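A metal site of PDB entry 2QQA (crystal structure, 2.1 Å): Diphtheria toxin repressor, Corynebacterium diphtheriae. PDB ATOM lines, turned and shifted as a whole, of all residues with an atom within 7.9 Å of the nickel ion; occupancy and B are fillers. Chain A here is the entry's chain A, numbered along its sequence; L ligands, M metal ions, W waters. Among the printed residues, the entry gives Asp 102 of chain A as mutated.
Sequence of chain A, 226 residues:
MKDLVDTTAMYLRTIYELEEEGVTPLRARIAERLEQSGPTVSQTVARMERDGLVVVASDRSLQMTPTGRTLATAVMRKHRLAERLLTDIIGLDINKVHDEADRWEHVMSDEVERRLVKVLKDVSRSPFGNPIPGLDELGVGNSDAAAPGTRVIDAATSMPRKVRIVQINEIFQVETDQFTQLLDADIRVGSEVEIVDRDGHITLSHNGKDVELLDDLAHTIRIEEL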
ATOM      1  N   ARG A  13      -1.915 -22.003  18.474  1.00  0.00           N
ATOM      2  CA  ARG A  13      -2.740 -23.002  19.123  1.00  0.00           C
ATOM      3  C   ARG A  13      -2.371 -24.443  18.747  1.00  0.00           C
ATOM      4  O   ARG A  13      -2.399 -25.334  19.587  1.00  0.00           O
ATOM      5  CB  ARG A  13      -4.271 -22.798  18.909  1.00  0.00           C
ATOM      6  CG  ARG A  13      -5.116 -23.795  19.834  1.00  0.00           C
ATOM      7  CD  ARG A  13      -6.653 -24.127  19.466  1.00  0.00           C
ATOM      8  NE  ARG A  13      -6.755 -25.271  18.578  1.00  0.00           N
ATOM      9  CZ  ARG A  13      -7.497 -25.306  17.485  1.00  0.00           C
ATOM     10  NH1 ARG A  13      -8.306 -24.292  17.195  1.00  0.00           N
ATOM     11  NH2 ARG A  13      -7.438 -26.388  16.678  1.00  0.00           N
ATOM     12  N   GLU A  17      -0.837 -27.445  21.105  1.00  0.00           N
ATOM     13  CA  GLU A  17      -1.479 -28.695  21.328  1.00  0.00           C
ATOM     14  C   GLU A  17      -0.532 -29.863  20.918  1.00  0.00           C
ATOM     15  O   GLU A  17      -0.481 -30.874  21.590  1.00  0.00           O
ATOM     16  CB  GLU A  17      -2.859 -28.729  20.667  1.00  0.00           C
ATOM     17  CG  GLU A  17      -2.842 -29.060  19.256  1.00  0.00           C
ATOM     18  CD  GLU A  17      -4.206 -28.765  18.599  1.00  0.00           C
ATOM     19  OE1 GLU A  17      -4.250 -28.821  17.375  1.00  0.00           O
ATOM     20  OE2 GLU A  17      -5.207 -28.478  19.334  1.00  0.00           O
ATOM     21  N   MET A  76      -5.712 -20.765  23.654  1.00  0.00           N
ATOM     22  CA  MET A  76      -6.147 -22.076  24.142  1.00  0.00           C
ATOM     23  C   MET A  76      -7.192 -21.934  25.236  1.00  0.00           C
ATOM     24  O   MET A  76      -8.176 -22.665  25.261  1.00  0.00           O
ATOM     25  CB  MET A  76      -4.947 -22.879  24.654  1.00  0.00           C
ATOM     26  CG  MET A  76      -5.273 -24.319  25.008  1.00  0.00           C
ATOM     27  SD  MET A  76      -5.581 -25.338  23.549  1.00  0.00           S
ATOM     28  CE  MET A  76      -7.370 -25.251  23.449  1.00  0.00           C
ATOM     29  N   HIS A  79     -10.343 -20.981  23.722  1.00  0.00           N
ATOM     30  CA  HIS A  79     -10.865 -22.139  22.994  1.00  0.00           C
ATOM     31  C   HIS A  79     -11.603 -23.211  23.840  1.00  0.00           C
ATOM     32  O   HIS A  79     -12.720 -23.642  23.521  1.00  0.00           O
ATOM     33  CB  HIS A  79      -9.711 -22.760  22.225  1.00  0.00           C
ATOM     34  CG  HIS A  79     -10.115 -23.974  21.500  1.00  0.00           C
ATOM     35  ND1 HIS A  79     -10.800 -23.920  20.314  1.00  0.00           N
ATOM     36  CD2 HIS A  79      -9.962 -25.278  21.798  1.00  0.00           C
ATOM     37  CE1 HIS A  79     -11.022 -25.154  19.878  1.00  0.00           C
ATOM     38  NE2 HIS A  79     -10.540 -25.994  20.772  1.00  0.00           N
ATOM     39  N   ARG A  80     -10.981 -23.552  24.963  1.00  0.00           N
ATOM     40  CA  ARG A  80     -11.501 -24.470  25.929  1.00  0.00           C
ATOM     41  C   ARG A  80     -12.655 -23.903  26.704  1.00  0.00           C
ATOM     42  O   ARG A  80     -13.559 -24.647  27.047  1.00  0.00           O
ATOM     43  CB  ARG A  80     -10.386 -24.989  26.875  1.00  0.00           C
ATOM     44  CG  ARG A  80      -9.370 -25.826  25.999  1.00  0.00           C
ATOM     45  CD  ARG A  80      -8.271 -26.581  26.779  1.00  0.00           C
ATOM     46  NE  ARG A  80      -7.574 -27.446  25.819  1.00  0.00           N
ATOM     47  CZ  ARG A  80      -6.279 -27.774  25.858  1.00  0.00           C
ATOM     48  NH1 ARG A  80      -5.513 -27.349  26.840  1.00  0.00           N
ATOM     49  NH2 ARG A  80      -5.761 -28.553  24.925  1.00  0.00           N
ATOM     50  N   GLU A  83     -15.549 -24.114  24.320  1.00  0.00           N
ATOM     51  CA  GLU A  83     -16.083 -25.500  24.272  1.00  0.00           C
ATOM     52  C   GLU A  83     -17.005 -25.892  25.482  1.00  0.00           C
ATOM     53  O   GLU A  83     -18.028 -26.495  25.315  1.00  0.00           O
ATOM     54  CB  GLU A  83     -14.961 -26.503  24.084  1.00  0.00           C
ATOM     55  CG  GLU A  83     -14.364 -26.396  22.728  1.00  0.00           C
ATOM     56  CD  GLU A  83     -13.076 -27.272  22.597  1.00  0.00           C
ATOM     57  OE1 GLU A  83     -12.295 -27.545  23.604  1.00  0.00           O
ATOM     58  OE2 GLU A  83     -12.824 -27.665  21.472  1.00  0.00           O
ATOM     59  N   VAL A  97     -18.850 -29.134  18.586  1.00  0.00           N
ATOM     60  CA  VAL A  97     -18.333 -28.193  19.571  1.00  0.00           C
ATOM     61  C   VAL A  97     -16.949 -27.660  19.240  1.00  0.00           C
ATOM     62  O   VAL A  97     -16.714 -26.428  19.330  1.00  0.00           O
ATOM     63  CB  VAL A  97     -18.500 -28.750  21.047  1.00  0.00           C
ATOM     64  CG1 VAL A  97     -17.570 -28.088  22.033  1.00  0.00           C
ATOM     65  CG2 VAL A  97     -19.983 -28.608  21.490  1.00  0.00           C
ATOM     66  N   HIS A  98     -16.020 -28.539  18.819  1.00  0.00           N
ATOM     67  CA  HIS A  98     -14.624 -28.128  18.688  1.00  0.00           C
ATOM     68  C   HIS A  98     -14.548 -27.172  17.476  1.00  0.00           C
ATOM     69  O   HIS A  98     -13.853 -26.166  17.517  1.00  0.00           O
ATOM     70  CB  HIS A  98     -13.587 -29.272  18.552  1.00  0.00           C
ATOM     71  CG  HIS A  98     -12.375 -28.842  17.789  1.00  0.00           C
ATOM     72  ND1 HIS A  98     -11.330 -28.164  18.382  1.00  0.00           N
ATOM     73  CD2 HIS A  98     -12.108 -28.868  16.459  1.00  0.00           C
ATOM     74  CE1 HIS A  98     -10.444 -27.846  17.458  1.00  0.00           C
ATOM     75  NE2 HIS A  98     -10.916 -28.221  16.274  1.00  0.00           N
ATOM     76  N   ASP A  99     -15.300 -27.508  16.407  1.00  0.00           N
ATOM     77  CA  ASP A  99     -15.207 -26.752  15.146  1.00  0.00           C
ATOM     78  C   ASP A  99     -15.799 -25.344  15.393  1.00  0.00           C
ATOM     79  O   ASP A  99     -15.299 -24.376  14.877  1.00  0.00           O
ATOM     80  CB  ASP A  99     -16.001 -27.421  14.038  1.00  0.00           C
ATOM     81  CG  ASP A  99     -15.264 -28.589  13.363  1.00  0.00           C
ATOM     82  OD1 ASP A  99     -13.981 -28.794  13.413  1.00  0.00           O
ATOM     83  OD2 ASP A  99     -16.049 -29.337  12.731  1.00  0.00           O
ATOM     84  N   ALA A 101     -15.769 -23.813  18.459  1.00  0.00           N
ATOM     85  CA  ALA A 101     -14.820 -23.138  19.319  1.00  0.00           C
ATOM     86  C   ALA A 101     -13.557 -22.736  18.571  1.00  0.00           C
ATOM     87  O   ALA A 101     -12.898 -21.762  18.928  1.00  0.00           O
ATOM     88  CB  ALA A 101     -14.539 -23.976  20.533  1.00  0.00           C
ATOM     89  N   ASP A 102     -13.253 -23.464  17.506  1.00  0.00           N
ATOM     90  CA  ASP A 102     -12.109 -23.207  16.664  1.00  0.00           C
ATOM     91  C   ASP A 102     -12.345 -21.790  16.030  1.00  0.00           C
ATOM     92  O   ASP A 102     -11.433 -21.101  15.804  1.00  0.00           O
ATOM     93  CB  ASP A 102     -12.137 -24.280  15.570  1.00  0.00           C
ATOM     94  CG  ASP A 102     -10.854 -24.421  14.817  1.00  0.00           C
ATOM     95  OD1 ASP A 102     -10.822 -25.266  13.894  1.00  0.00           O
ATOM     96  OD2 ASP A 102      -9.848 -23.734  15.056  1.00  0.00           O
ATOM     97  N   GLU A 105     -12.641 -18.789  19.346  1.00  0.00           N
ATOM     98  CA  GLU A 105     -11.429 -18.526  20.135  1.00  0.00           C
ATOM     99  C   GLU A 105     -10.670 -17.256  19.681  1.00  0.00           C
ATOM    100  O   GLU A 105      -9.944 -16.682  20.478  1.00  0.00           O
ATOM    101  CB  GLU A 105     -10.444 -19.707  20.104  1.00  0.00           C
ATOM    102  CG  GLU A 105      -9.806 -19.904  18.692  1.00  0.00           C
ATOM    103  CD  GLU A 105      -9.060 -21.269  18.619  1.00  0.00           C
ATOM    104  OE1 GLU A 105      -8.797 -21.859  19.636  1.00  0.00           O
ATOM    105  OE2 GLU A 105      -8.734 -21.743  17.574  1.00  0.00           O
ATOM    106  N   SER A 126     -11.433 -28.810  29.449  1.00  0.00           N
ATOM    107  CA  SER A 126     -12.385 -28.768  28.356  1.00  0.00           C
ATOM    108  C   SER A 126     -13.186 -30.062  28.336  1.00  0.00           C
ATOM    109  O   SER A 126     -12.797 -31.050  29.051  1.00  0.00           O
ATOM    110  CB  SER A 126     -11.651 -28.614  27.005  1.00  0.00           C
ATOM    111  OG  SER A 126     -11.001 -29.825  26.654  1.00  0.00           O
ATOM    112  N   PRO A 127     -14.257 -30.097  27.504  1.00  0.00           N
ATOM    113  CA  PRO A 127     -15.037 -31.374  27.466  1.00  0.00           C
ATOM    114  C   PRO A 127     -14.225 -32.507  26.848  1.00  0.00           C
ATOM    115  O   PRO A 127     -14.640 -33.635  26.816  1.00  0.00           O
ATOM    116  CB  PRO A 127     -16.268 -31.003  26.598  1.00  0.00           C
ATOM    117  CG  PRO A 127     -16.324 -29.487  26.533  1.00  0.00           C
ATOM    118  CD  PRO A 127     -14.881 -29.075  26.622  1.00  0.00           C
ATOM    119  N   PHE A 128     -13.022 -32.193  26.361  1.00  0.00           N
ATOM    120  CA  PHE A 128     -12.245 -33.150  25.611  1.00  0.00           C
ATOM    121  C   PHE A 128     -11.018 -33.558  26.383  1.00  0.00           C
ATOM    122  O   PHE A 128     -10.062 -34.120  25.826  1.00  0.00           O
ATOM    123  CB  PHE A 128     -11.874 -32.624  24.240  1.00  0.00           C
ATOM    124  CG  PHE A 128     -13.060 -32.170  23.451  1.00  0.00           C
ATOM    125  CD1 PHE A 128     -13.206 -30.834  23.157  1.00  0.00           C
ATOM    126  CD2 PHE A 128     -14.067 -33.080  23.114  1.00  0.00           C
ATOM    127  CE1 PHE A 128     -14.329 -30.351  22.441  1.00  0.00           C
ATOM    128  CE2 PHE A 128     -15.244 -32.640  22.419  1.00  0.00           C
ATOM    129  CZ  PHE A 128     -15.342 -31.223  22.088  1.00  0.00           C
ATOM    130  N   ASN A 130      -8.771 -31.895  28.423  1.00  0.00           N
ATOM    131  CA  ASN A 130      -7.501 -31.215  28.677  1.00  0.00           C
ATOM    132  C   ASN A 130      -7.696 -30.036  29.601  1.00  0.00           C
ATOM    133  O   ASN A 130      -8.704 -29.280  29.455  1.00  0.00           O
ATOM    134  CB  ASN A 130      -6.855 -30.745  27.390  1.00  0.00           C
ATOM    135  CG  ASN A 130      -6.823 -31.822  26.381  1.00  0.00           C
ATOM    136  OD1 ASN A 130      -6.086 -32.733  26.536  1.00  0.00           O
ATOM    137  ND2 ASN A 130      -7.687 -31.751  25.365  1.00  0.00           N
HETATM  138  P1  LIG L   1      -9.176 -29.467  23.179  1.00  0.00           P
HETATM  139  O1  LIG L   1      -7.819 -28.929  22.724  1.00  0.00           O
HETATM  140  O2  LIG L   1      -9.281 -29.608  24.635  1.00  0.00           O
HETATM  141  O3  LIG L   1      -9.524 -30.788  22.509  1.00  0.00           O
HETATM  142  O4  LIG L   1     -10.153 -28.458  22.745  1.00  0.00           O
HETATM  143 NI    NI M   1     -10.892 -28.152  20.653  1.00  0.00          NI
HETATM  144  O   HOH W   1      -8.761 -28.564  20.066  1.00  0.00           O
HETATM  145  O   HOH W   2     -11.148 -30.449  20.673  1.00  0.00           O
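A ring nitrogen (ND1) of His 79 is in hydrogen-bond range of the backbone carbonyl oxygen of Ala 101 (3.3 Å). A ring nitrogen (ND1) of His 79 lies close to the side-chain carboxylate (OE1) of Glu 105, at 3.0 Å.
Three residues have an atom within 4 Å of the nickel ion: His 79, Glu 83 and His 98. The nearest printed residue that does not touch the nickel ion is Phe 128 (4.3 Å).
The nickel ion is bound by OE2 of Glu 83, NE2 of His 79, O4 of the ligand, water W1, water W2 and ND1 of His 98.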
